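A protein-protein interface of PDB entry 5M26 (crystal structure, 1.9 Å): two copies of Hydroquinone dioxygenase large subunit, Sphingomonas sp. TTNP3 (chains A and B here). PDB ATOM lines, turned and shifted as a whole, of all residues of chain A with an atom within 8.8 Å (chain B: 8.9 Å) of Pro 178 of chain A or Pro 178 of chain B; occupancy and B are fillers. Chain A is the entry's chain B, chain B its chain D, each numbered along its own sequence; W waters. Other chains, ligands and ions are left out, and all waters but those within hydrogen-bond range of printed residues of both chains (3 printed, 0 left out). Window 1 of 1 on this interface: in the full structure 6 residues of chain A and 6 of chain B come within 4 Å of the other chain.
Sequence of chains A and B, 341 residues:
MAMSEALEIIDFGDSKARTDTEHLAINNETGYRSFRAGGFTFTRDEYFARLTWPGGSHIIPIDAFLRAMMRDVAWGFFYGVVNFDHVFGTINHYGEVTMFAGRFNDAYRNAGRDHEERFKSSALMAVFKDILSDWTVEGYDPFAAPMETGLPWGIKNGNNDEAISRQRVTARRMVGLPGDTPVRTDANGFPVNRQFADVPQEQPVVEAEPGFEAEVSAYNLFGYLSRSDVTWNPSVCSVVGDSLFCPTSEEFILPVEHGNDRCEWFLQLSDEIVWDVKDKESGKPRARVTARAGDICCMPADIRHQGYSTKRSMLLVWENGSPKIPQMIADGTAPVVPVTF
Arg 172 of chain A touches Arg 172 of chain B.
NH1 of Arg 172 of chain A touches NH1 of Arg 173 of chain B, at 3.6 Å.
Arg 173 of chain A touches Arg 172 of chain B (NH1 to NH2, 3.6 Å).
Pro 178 of chain A touches Pro 178 of chain B (CB to C, 3.9 Å).
Pro 178 of chain A touches Gly 179 of chain B (CB to N, 3.7 Å).
CA of Gly 179 of chain A touches CB of Pro 178 of chain B (3.9 Å).
Gly 179 of chain A touches Ala 214 of chain B.
Ala 214 of chain A touches Gly 179 of chain B.
The backbone NH of Arg 172 of chain A sits at hydrogen-bond distance from the side-chain carboxylate of Asp 180 of chain A, 2.7 Å away.
The backbone NH (N) of Arg 173 of chain A lies within hydrogen-bond range of the side-chain carboxylate (OD2) of Asp 180 of chain A (2.6 Å).
The backbone NH of Arg 173 of chain B lies within hydrogen-bond range of the side-chain carboxylate of Asp 180 of chain B, 2.8 Å away.
The side-chain carboxylate (OD1) of Asp 180 of chain B sits at hydrogen-bond distance from the backbone NH (N) of Arg 172 of chain B, 2.8 Å away.
NH2 of Arg 173 of chain A is in salt-bridge range of OE2 of Glu 215 of chain A.
The guanidinium group (NH2) of Arg 173 of chain B lies within salt-bridge range of the side-chain carboxylate (OE1) of Glu 215 of chain B.
Of the 17 printed residues of chain B, 6 touch a printed residue of chain A.
Among the printed residues, 10 pairs touch across the chains.
Arg 172 of chain A touches Arg 173 of chain B, and with the chains exchanged Arg 173 of chain A touches Arg 172 of chain B.
Arg 172 of chain A touches Glu 215 of chain B, and with the chains exchanged Glu 215 of chain A touches Arg 172 of chain B.
Pro 178 of chain A touches its own counterpart, Pro 178 of chain B.
Pro 178 of chain A touches Gly 179 of chain B, and with the chains exchanged Gly 179 of chain A touches Pro 178 of chain B.
Positions printed for both chains: 172, 173, 174, 175, 176, 177, 178, 179, 180, 181, 182, 212, 213, 214, 215, 216 and 217.
Of the 10 pairs that touch across the chains among the printed residues, 10 have their exchanged pair printed and touching as well.
Pro 178 of chain A touches two residues of chain B.
Pro 178 of chain B touches just these residues of chain A: Pro 178 (3.9 Å) and Gly 179 (3.9 Å).
Of chain B, only Pro 178 (3.9 Å) and Ala 214 (3.2 Å) come within 4 Å of Gly 179 of chain A.
Of the printed residues of chain A, Gly 179 of chain B touches Pro 178 (3.7 Å) and Ala 214 (3.2 Å).
Of the printed residues of chain A, Arg 172 of chain B touches Arg 172, Arg 173 and Glu 215.
Of the printed residues of chain A, Arg 173 of chain B touches Arg 172 (3.6 Å).
Of the printed residues of chain B, Glu 215 of chain A touches Arg 172 (3.8 Å).
Phe 212 of chain B touches none of the printed residues of chain A.
The nearest residue of chain A that does not touch Pro 178 of chain B is Ala 214 of chain A (5.8 Å).
Water W2 bridges NH1 of Arg 172 of chain A (2.8 Å) and NH2 of Arg 172 of chain B (3.2 Å).
Water W3 bridges the guanidinium group of Arg 172 of chain B and the guanidinium group of Arg 173 of chain A.
Water W1 bridges the guanidinium group of Arg 172 of chain A and the guanidinium group of Arg 173 of chain B.
NE of Arg 172 of chain A lies within salt-bridge range of OE1 of Glu 215 of chain B.
The side-chain carboxylate (OE2) of Glu 215 of chain A is in salt-bridge range of the guanidinium group (NE) of Arg 172 of chain B, 3.8 Å away.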
ATOM      1  N   ARG A 172      -3.189 -21.879   5.645  1.00  0.00           N
ATOM      2  CA  ARG A 172      -4.043 -20.875   5.028  1.00  0.00           C
ATOM      3  C   ARG A 172      -3.275 -19.543   4.900  1.00  0.00           C
ATOM      4  O   ARG A 172      -3.441 -18.824   3.929  1.00  0.00           O
ATOM      5  CB  ARG A 172      -5.313 -20.657   5.888  1.00  0.00           C
ATOM      6  CG  ARG A 172      -6.149 -19.455   5.441  1.00  0.00           C
ATOM      7  CD  ARG A 172      -7.341 -19.100   6.346  1.00  0.00           C
ATOM      8  NE  ARG A 172      -7.915 -17.805   5.954  1.00  0.00           N
ATOM      9  CZ  ARG A 172      -7.583 -16.618   6.486  1.00  0.00           C
ATOM     10  NH1 ARG A 172      -8.160 -15.506   6.026  1.00  0.00           N
ATOM     11  NH2 ARG A 172      -6.679 -16.522   7.474  1.00  0.00           N
ATOM     12  N   ARG A 173      -2.450 -19.202   5.889  1.00  0.00           N
ATOM     13  CA  ARG A 173      -1.709 -17.957   5.846  1.00  0.00           C
ATOM     14  C   ARG A 173      -0.260 -18.261   6.217  1.00  0.00           C
ATOM     15  O   ARG A 173       0.651 -18.035   5.421  1.00  0.00           O
ATOM     16  CB  ARG A 173      -2.370 -16.899   6.753  1.00  0.00           C
ATOM     17  CG  ARG A 173      -1.673 -15.523   6.784  1.00  0.00           C
ATOM     18  CD  ARG A 173      -2.534 -14.533   7.574  1.00  0.00           C
ATOM     19  NE  ARG A 173      -2.080 -13.136   7.463  1.00  0.00           N
ATOM     20  CZ  ARG A 173      -2.308 -12.217   8.396  1.00  0.00           C
ATOM     21  NH1 ARG A 173      -2.940 -12.558   9.517  1.00  0.00           N
ATOM     22  NH2 ARG A 173      -1.910 -10.968   8.226  1.00  0.00           N
ATOM     23  N   MET A 174      -0.062 -18.833   7.405  1.00  0.00           N
ATOM     24  CA  MET A 174       1.251 -19.282   7.840  1.00  0.00           C
ATOM     25  C   MET A 174       1.100 -20.299   8.952  1.00  0.00           C
ATOM     26  O   MET A 174       0.189 -20.196   9.773  1.00  0.00           O
ATOM     27  CB  MET A 174       2.107 -18.117   8.365  1.00  0.00           C
ATOM     28  CG  MET A 174       3.569 -18.474   8.607  1.00  0.00           C
ATOM     29  SD  MET A 174       4.534 -17.035   9.134  1.00  0.00           S
ATOM     30  CE  MET A 174       4.311 -17.108  10.911  1.00  0.00           C
ATOM     31  N   VAL A 175       2.006 -21.271   8.944  1.00  0.00           N
ATOM     32  CA  VAL A 175       2.163 -22.221  10.027  1.00  0.00           C
ATOM     33  C   VAL A 175       2.175 -21.471  11.366  1.00  0.00           C
ATOM     34  O   VAL A 175       2.856 -20.464  11.517  1.00  0.00           O
ATOM     35  CB  VAL A 175       3.461 -23.055   9.857  1.00  0.00           C
ATOM     36  CG1 VAL A 175       3.701 -23.972  11.056  1.00  0.00           C
ATOM     37  CG2 VAL A 175       3.409 -23.875   8.573  1.00  0.00           C
ATOM     38  N   GLY A 176       1.381 -21.947  12.321  1.00  0.00           N
ATOM     39  CA  GLY A 176       1.533 -21.495  13.688  1.00  0.00           C
ATOM     40  C   GLY A 176       0.634 -20.347  14.075  1.00  0.00           C
ATOM     41  O   GLY A 176       0.546 -20.022  15.272  1.00  0.00           O
ATOM     42  N   LEU A 177      -0.018 -19.719  13.082  1.00  0.00           N
ATOM     43  CA  LEU A 177      -0.926 -18.605  13.326  1.00  0.00           C
ATOM     44  C   LEU A 177      -2.199 -19.135  14.003  1.00  0.00           C
ATOM     45  O   LEU A 177      -2.532 -20.292  13.812  1.00  0.00           O
ATOM     46  CB  LEU A 177      -1.285 -17.907  12.002  1.00  0.00           C
ATOM     47  CG  LEU A 177      -0.247 -16.889  11.486  1.00  0.00           C
ATOM     48  CD1 LEU A 177      -0.613 -16.529  10.061  1.00  0.00           C
ATOM     49  CD2 LEU A 177      -0.258 -15.635  12.331  1.00  0.00           C
ATOM     50  N   PRO A 178      -2.911 -18.300  14.783  1.00  0.00           N
ATOM     51  CA  PRO A 178      -4.130 -18.853  15.436  1.00  0.00           C
ATOM     52  C   PRO A 178      -5.117 -19.411  14.435  1.00  0.00           C
ATOM     53  O   PRO A 178      -5.452 -18.758  13.445  1.00  0.00           O
ATOM     54  CB  PRO A 178      -4.739 -17.640  16.154  1.00  0.00           C
ATOM     55  CG  PRO A 178      -3.574 -16.706  16.363  1.00  0.00           C
ATOM     56  CD  PRO A 178      -2.683 -16.889  15.156  1.00  0.00           C
ATOM     57  N   GLY A 179      -5.570 -20.637  14.670  1.00  0.00           N
ATOM     58  CA  GLY A 179      -6.511 -21.243  13.751  1.00  0.00           C
ATOM     59  C   GLY A 179      -5.871 -21.829  12.492  1.00  0.00           C
ATOM     60  O   GLY A 179      -6.575 -22.454  11.699  1.00  0.00           O
ATOM     61  N   ASP A 180      -4.561 -21.616  12.278  1.00  0.00           N
ATOM     62  CA  ASP A 180      -3.888 -22.156  11.080  1.00  0.00           C
ATOM     63  C   ASP A 180      -3.189 -23.482  11.398  1.00  0.00           C
ATOM     64  O   ASP A 180      -3.193 -23.944  12.543  1.00  0.00           O
ATOM     65  CB  ASP A 180      -2.884 -21.123  10.511  1.00  0.00           C
ATOM     66  CG  ASP A 180      -2.845 -21.110   8.972  1.00  0.00           C
ATOM     67  OD1 ASP A 180      -2.924 -22.207   8.347  1.00  0.00           O
ATOM     68  OD2 ASP A 180      -2.699 -20.006   8.378  1.00  0.00           O
ATOM     69  N   THR A 181      -2.536 -24.073  10.404  1.00  0.00           N
ATOM     70  CA  THR A 181      -1.893 -25.363  10.593  1.00  0.00           C
ATOM     71  C   THR A 181      -0.771 -25.259  11.652  1.00  0.00           C
ATOM     72  O   THR A 181      -0.048 -24.242  11.713  1.00  0.00           O
ATOM     73  CB  THR A 181      -1.403 -25.946   9.249  1.00  0.00           C
ATOM     74  OG1 THR A 181      -1.000 -27.292   9.461  1.00  0.00           O
ATOM     75  CG2 THR A 181      -0.218 -25.168   8.728  1.00  0.00           C
ATOM     76  N   PRO A 182      -0.665 -26.259  12.539  1.00  0.00           N
ATOM     77  CA  PRO A 182       0.187 -26.061  13.725  1.00  0.00           C
ATOM     78  C   PRO A 182       1.668 -26.360  13.507  1.00  0.00           C
ATOM     79  O   PRO A 182       2.019 -27.091  12.590  1.00  0.00           O
ATOM     80  CB  PRO A 182      -0.376 -27.065  14.738  1.00  0.00           C
ATOM     81  CG  PRO A 182      -1.000 -28.139  13.885  1.00  0.00           C
ATOM     82  CD  PRO A 182      -1.575 -27.410  12.695  1.00  0.00           C
ATOM     83  N   PHE A 212      -1.827  -7.505  20.315  1.00  0.00           N
ATOM     84  CA  PHE A 212      -1.282  -7.869  19.015  1.00  0.00           C
ATOM     85  C   PHE A 212      -0.756  -9.307  18.912  1.00  0.00           C
ATOM     86  O   PHE A 212      -0.059  -9.646  17.952  1.00  0.00           O
ATOM     87  CB  PHE A 212      -0.178  -6.881  18.623  1.00  0.00           C
ATOM     88  CG  PHE A 212      -0.669  -5.481  18.417  1.00  0.00           C
ATOM     89  CD1 PHE A 212      -1.437  -5.160  17.295  1.00  0.00           C
ATOM     90  CD2 PHE A 212      -0.363  -4.480  19.340  1.00  0.00           C
ATOM     91  CE1 PHE A 212      -1.886  -3.863  17.096  1.00  0.00           C
ATOM     92  CE2 PHE A 212      -0.817  -3.183  19.149  1.00  0.00           C
ATOM     93  CZ  PHE A 212      -1.579  -2.875  18.027  1.00  0.00           C
ATOM     94  N   GLU A 213      -1.102 -10.161  19.865  1.00  0.00           N
ATOM     95  CA  GLU A 213      -0.540 -11.518  19.862  1.00  0.00           C
ATOM     96  C   GLU A 213      -0.899 -12.348  18.633  1.00  0.00           C
ATOM     97  O   GLU A 213      -0.117 -13.202  18.237  1.00  0.00           O
ATOM     98  CB  GLU A 213      -0.739 -12.281  21.189  1.00  0.00           C
ATOM     99  CG  GLU A 213      -2.007 -12.017  21.966  1.00  0.00           C
ATOM    100  CD  GLU A 213      -2.092 -10.613  22.553  1.00  0.00           C
ATOM    101  OE1 GLU A 213      -2.913  -9.834  22.035  1.00  0.00           O
ATOM    102  OE2 GLU A 213      -1.364 -10.293  23.525  1.00  0.00           O
ATOM    103  N   ALA A 214      -2.046 -12.073  18.014  1.00  0.00           N
ATOM    104  CA  ALA A 214      -2.464 -12.788  16.802  1.00  0.00           C
ATOM    105  C   ALA A 214      -1.653 -12.467  15.552  1.00  0.00           C
ATOM    106  O   ALA A 214      -1.666 -13.259  14.605  1.00  0.00           O
ATOM    107  CB  ALA A 214      -3.935 -12.539  16.512  1.00  0.00           C
ATOM    108  N   GLU A 215      -0.973 -11.316  15.511  1.00  0.00           N
ATOM    109  CA  GLU A 215      -0.260 -10.932  14.273  1.00  0.00           C
ATOM    110  C   GLU A 215       1.245 -10.709  14.382  1.00  0.00           C
ATOM    111  O   GLU A 215       1.879 -10.232  13.449  1.00  0.00           O
ATOM    112  CB  GLU A 215      -0.951  -9.765  13.567  1.00  0.00           C
ATOM    113  CG  GLU A 215      -2.106 -10.246  12.694  1.00  0.00           C
ATOM    114  CD  GLU A 215      -2.541  -9.246  11.642  1.00  0.00           C
ATOM    115  OE1 GLU A 215      -2.273  -8.016  11.783  1.00  0.00           O
ATOM    116  OE2 GLU A 215      -3.168  -9.702  10.660  1.00  0.00           O
ATOM    117  N   VAL A 216       1.805 -11.056  15.530  1.00  0.00           N
ATOM    118  CA  VAL A 216       3.239 -11.086  15.715  1.00  0.00           C
ATOM    119  C   VAL A 216       3.518 -12.579  15.804  1.00  0.00           C
ATOM    120  O   VAL A 216       3.274 -13.200  16.836  1.00  0.00           O
ATOM    121  CB  VAL A 216       3.657 -10.338  16.988  1.00  0.00           C
ATOM    122  CG1 VAL A 216       5.180 -10.339  17.148  1.00  0.00           C
ATOM    123  CG2 VAL A 216       3.135  -8.908  16.939  1.00  0.00           C
ATOM    124  N   SER A 217       4.018 -13.160  14.718  1.00  0.00           N
ATOM    125  CA  SER A 217       4.109 -14.607  14.640  1.00  0.00           C
ATOM    126  C   SER A 217       5.359 -15.059  13.878  1.00  0.00           C
ATOM    127  O   SER A 217       5.687 -14.526  12.814  1.00  0.00           O
ATOM    128  CB  SER A 217       2.852 -15.169  14.000  1.00  0.00           C
ATOM    129  OG  SER A 217       2.811 -16.580  14.119  1.00  0.00           O
ATOM    130  N   ARG B 172     -10.621  -8.033  12.258  1.00  0.00           N
ATOM    131  CA  ARG B 172      -9.805  -8.176  11.050  1.00  0.00           C
ATOM    132  C   ARG B 172     -10.597  -8.908   9.948  1.00  0.00           C
ATOM    133  O   ARG B 172     -10.471  -8.602   8.781  1.00  0.00           O
ATOM    134  CB  ARG B 172      -8.511  -8.934  11.353  1.00  0.00           C
ATOM    135  CG  ARG B 172      -7.801  -9.427  10.091  1.00  0.00           C
ATOM    136  CD  ARG B 172      -6.809 -10.561  10.335  1.00  0.00           C
ATOM    137  NE  ARG B 172      -6.291 -11.137   9.086  1.00  0.00           N
ATOM    138  CZ  ARG B 172      -6.505 -12.387   8.665  1.00  0.00           C
ATOM    139  NH1 ARG B 172      -7.236 -13.242   9.389  1.00  0.00           N
ATOM    140  NH2 ARG B 172      -5.970 -12.792   7.510  1.00  0.00           N
ATOM    141  N   ARG B 173     -11.413  -9.882  10.333  1.00  0.00           N
ATOM    142  CA  ARG B 173     -12.215 -10.644   9.401  1.00  0.00           C
ATOM    143  C   ARG B 173     -13.642 -10.787   9.981  1.00  0.00           C
ATOM    144  O   ARG B 173     -14.608 -10.389   9.328  1.00  0.00           O
ATOM    145  CB  ARG B 173     -11.568 -12.004   9.186  1.00  0.00           C
ATOM    146  CG  ARG B 173     -12.201 -12.859   8.109  1.00  0.00           C
ATOM    147  CD  ARG B 173     -11.416 -14.164   7.988  1.00  0.00           C
ATOM    148  NE  ARG B 173     -11.856 -14.970   6.852  1.00  0.00           N
ATOM    149  CZ  ARG B 173     -11.617 -16.276   6.706  1.00  0.00           C
ATOM    150  NH1 ARG B 173     -10.977 -16.967   7.637  1.00  0.00           N
ATOM    151  NH2 ARG B 173     -12.060 -16.900   5.628  1.00  0.00           N
ATOM    152  N   MET B 174     -13.758 -11.324  11.205  1.00  0.00           N
ATOM    153  CA  MET B 174     -15.076 -11.441  11.907  1.00  0.00           C
ATOM    154  C   MET B 174     -14.912 -11.670  13.408  1.00  0.00           C
ATOM    155  O   MET B 174     -14.042 -12.421  13.837  1.00  0.00           O
ATOM    156  CB  MET B 174     -15.956 -12.553  11.310  1.00  0.00           C
ATOM    157  CG  MET B 174     -17.485 -12.472  11.612  1.00  0.00           C
ATOM    158  SD  MET B 174     -18.462 -13.904  11.028  1.00  0.00           S
ATOM    159  CE  MET B 174     -17.833 -15.185  12.111  1.00  0.00           C
ATOM    160  N   VAL B 175     -15.789 -11.048  14.204  1.00  0.00           N
ATOM    161  CA  VAL B 175     -15.859 -11.323  15.616  1.00  0.00           C
ATOM    162  C   VAL B 175     -15.853 -12.829  15.839  1.00  0.00           C
ATOM    163  O   VAL B 175     -16.526 -13.587  15.107  1.00  0.00           O
ATOM    164  CB  VAL B 175     -17.165 -10.744  16.249  1.00  0.00           C
ATOM    165  CG1 VAL B 175     -17.289 -11.202  17.697  1.00  0.00           C
ATOM    166  CG2 VAL B 175     -17.163  -9.218  16.208  1.00  0.00           C
ATOM    167  N   GLY B 176     -15.100 -13.271  16.852  1.00  0.00           N
ATOM    168  CA  GLY B 176     -15.210 -14.666  17.296  1.00  0.00           C
ATOM    169  C   GLY B 176     -14.263 -15.663  16.650  1.00  0.00           C
ATOM    170  O   GLY B 176     -14.073 -16.784  17.184  1.00  0.00           O
ATOM    171  N   LEU B 177     -13.686 -15.304  15.506  1.00  0.00           N
ATOM    172  CA  LEU B 177     -12.719 -16.173  14.821  1.00  0.00           C
ATOM    173  C   LEU B 177     -11.428 -16.289  15.630  1.00  0.00           C
ATOM    174  O   LEU B 177     -11.100 -15.376  16.401  1.00  0.00           O
ATOM    175  CB  LEU B 177     -12.411 -15.652  13.420  1.00  0.00           C
ATOM    176  CG  LEU B 177     -13.529 -15.903  12.391  1.00  0.00           C
ATOM    177  CD1 LEU B 177     -13.256 -15.111  11.122  1.00  0.00           C
ATOM    178  CD2 LEU B 177     -13.632 -17.397  12.081  1.00  0.00           C
ATOM    179  N   PRO B 178     -10.677 -17.390  15.447  1.00  0.00           N
ATOM    180  CA  PRO B 178      -9.430 -17.540  16.208  1.00  0.00           C
ATOM    181  C   PRO B 178      -8.464 -16.396  15.903  1.00  0.00           C
ATOM    182  O   PRO B 178      -8.255 -16.052  14.735  1.00  0.00           O
ATOM    183  CB  PRO B 178      -8.855 -18.862  15.700  1.00  0.00           C
ATOM    184  CG  PRO B 178     -10.012 -19.591  15.102  1.00  0.00           C
ATOM    185  CD  PRO B 178     -10.875 -18.507  14.500  1.00  0.00           C
ATOM    186  N   GLY B 179      -7.907 -15.814  16.957  1.00  0.00           N
ATOM    187  CA  GLY B 179      -7.014 -14.666  16.837  1.00  0.00           C
ATOM    188  C   GLY B 179      -7.732 -13.351  16.582  1.00  0.00           C
ATOM    189  O   GLY B 179      -7.102 -12.306  16.624  1.00  0.00           O
ATOM    190  N   ASP B 180      -9.044 -13.366  16.318  1.00  0.00           N
ATOM    191  CA  ASP B 180      -9.747 -12.106  15.991  1.00  0.00           C
ATOM    192  C   ASP B 180     -10.418 -11.492  17.225  1.00  0.00           C
ATOM    193  O   ASP B 180     -10.287 -12.016  18.337  1.00  0.00           O
ATOM    194  CB  ASP B 180     -10.776 -12.318  14.881  1.00  0.00           C
ATOM    195  CG  ASP B 180     -10.872 -11.124  13.909  1.00  0.00           C
ATOM    196  OD1 ASP B 180     -10.816  -9.928  14.319  1.00  0.00           O
ATOM    197  OD2 ASP B 180     -11.053 -11.378  12.708  1.00  0.00           O
ATOM    198  N   THR B 181     -11.106 -10.366  17.042  1.00  0.00           N
ATOM    199  CA  THR B 181     -11.720  -9.680  18.175  1.00  0.00           C
ATOM    200  C   THR B 181     -12.777 -10.605  18.807  1.00  0.00           C
ATOM    201  O   THR B 181     -13.580 -11.174  18.091  1.00  0.00           O
ATOM    202  CB  THR B 181     -12.278  -8.285  17.785  1.00  0.00           C
ATOM    203  OG1 THR B 181     -12.614  -7.553  18.972  1.00  0.00           O
ATOM    204  CG2 THR B 181     -13.498  -8.374  16.900  1.00  0.00           C
ATOM    205  N   PRO B 182     -12.749 -10.774  20.146  1.00  0.00           N
ATOM    206  CA  PRO B 182     -13.581 -11.772  20.837  1.00  0.00           C
ATOM    207  C   PRO B 182     -15.072 -11.418  20.961  1.00  0.00           C
ATOM    208  O   PRO B 182     -15.460 -10.242  20.888  1.00  0.00           O
ATOM    209  CB  PRO B 182     -12.960 -11.794  22.248  1.00  0.00           C
ATOM    210  CG  PRO B 182     -12.455 -10.402  22.421  1.00  0.00           C
ATOM    211  CD  PRO B 182     -11.825 -10.115  21.085  1.00  0.00           C
ATOM    212  N   PHE B 212     -11.920 -28.324  10.417  1.00  0.00           N
ATOM    213  CA  PHE B 212     -12.490 -27.093   9.869  1.00  0.00           C
ATOM    214  C   PHE B 212     -12.992 -26.118  10.944  1.00  0.00           C
ATOM    215  O   PHE B 212     -13.742 -25.179  10.634  1.00  0.00           O
ATOM    216  CB  PHE B 212     -13.588 -27.421   8.848  1.00  0.00           C
ATOM    217  CG  PHE B 212     -13.100 -28.211   7.660  1.00  0.00           C
ATOM    218  CD1 PHE B 212     -12.316 -27.612   6.687  1.00  0.00           C
ATOM    219  CD2 PHE B 212     -13.416 -29.557   7.523  1.00  0.00           C
ATOM    220  CE1 PHE B 212     -11.875 -28.324   5.583  1.00  0.00           C
ATOM    221  CE2 PHE B 212     -12.952 -30.286   6.431  1.00  0.00           C
ATOM    222  CZ  PHE B 212     -12.190 -29.665   5.458  1.00  0.00           C
ATOM    223  N   GLU B 213     -12.564 -26.340  12.193  1.00  0.00           N
ATOM    224  CA  GLU B 213     -12.978 -25.521  13.353  1.00  0.00           C
ATOM    225  C   GLU B 213     -12.751 -24.024  13.125  1.00  0.00           C
ATOM    226  O   GLU B 213     -13.547 -23.203  13.561  1.00  0.00           O
ATOM    227  CB  GLU B 213     -12.230 -25.935  14.626  1.00  0.00           C
ATOM    228  CG  GLU B 213     -12.505 -27.347  15.114  1.00  0.00           C
ATOM    229  CD  GLU B 213     -11.745 -28.418  14.329  1.00  0.00           C
ATOM    230  OE1 GLU B 213     -12.106 -29.602  14.495  1.00  0.00           O
ATOM    231  OE2 GLU B 213     -10.819 -28.098  13.535  1.00  0.00           O
ATOM    232  N   ALA B 214     -11.657 -23.673  12.448  1.00  0.00           N
ATOM    233  CA  ALA B 214     -11.286 -22.267  12.295  1.00  0.00           C
ATOM    234  C   ALA B 214     -12.112 -21.523  11.256  1.00  0.00           C
ATOM    235  O   ALA B 214     -12.122 -20.290  11.267  1.00  0.00           O
ATOM    236  CB  ALA B 214      -9.783 -22.118  11.992  1.00  0.00           C
ATOM    237  N   GLU B 215     -12.777 -22.235  10.345  1.00  0.00           N
ATOM    238  CA  GLU B 215     -13.544 -21.543   9.302  1.00  0.00           C
ATOM    239  C   GLU B 215     -15.038 -21.827   9.300  1.00  0.00           C
ATOM    240  O   GLU B 215     -15.740 -21.441   8.371  1.00  0.00           O
ATOM    241  CB  GLU B 215     -12.968 -21.798   7.928  1.00  0.00           C
ATOM    242  CG  GLU B 215     -11.588 -21.177   7.769  1.00  0.00           C
ATOM    243  CD  GLU B 215     -11.314 -20.770   6.348  1.00  0.00           C
ATOM    244  OE1 GLU B 215     -10.955 -19.590   6.131  1.00  0.00           O
ATOM    245  OE2 GLU B 215     -11.463 -21.639   5.459  1.00  0.00           O
ATOM    246  N   VAL B 216     -15.512 -22.501  10.333  1.00  0.00           N
ATOM    247  CA  VAL B 216     -16.950 -22.693  10.538  1.00  0.00           C
ATOM    248  C   VAL B 216     -17.268 -21.858  11.776  1.00  0.00           C
ATOM    249  O   VAL B 216     -16.931 -22.234  12.887  1.00  0.00           O
ATOM    250  CB  VAL B 216     -17.287 -24.190  10.697  1.00  0.00           C
ATOM    251  CG1 VAL B 216     -18.761 -24.383  11.057  1.00  0.00           C
ATOM    252  CG2 VAL B 216     -16.948 -24.960   9.413  1.00  0.00           C
ATOM    253  N   SER B 217     -17.850 -20.681  11.578  1.00  0.00           N
ATOM    254  CA  SER B 217     -17.910 -19.716  12.656  1.00  0.00           C
ATOM    255  C   SER B 217     -19.140 -18.841  12.546  1.00  0.00           C
ATOM    256  O   SER B 217     -19.512 -18.412  11.449  1.00  0.00           O
ATOM    257  CB  SER B 217     -16.645 -18.834  12.633  1.00  0.00           C
ATOM    258  OG  SER B 217     -16.548 -18.025  13.794  1.00  0.00           O
HETATM  259  O   HOH W   1     -10.185 -14.384   3.979  1.00  0.00           O
HETATM  260  O   HOH W   2      -5.579 -14.987   5.204  1.00  0.00           O
HETATM  261  O   HOH W   3      -4.742  -9.340   7.106  1.00  0.00           O
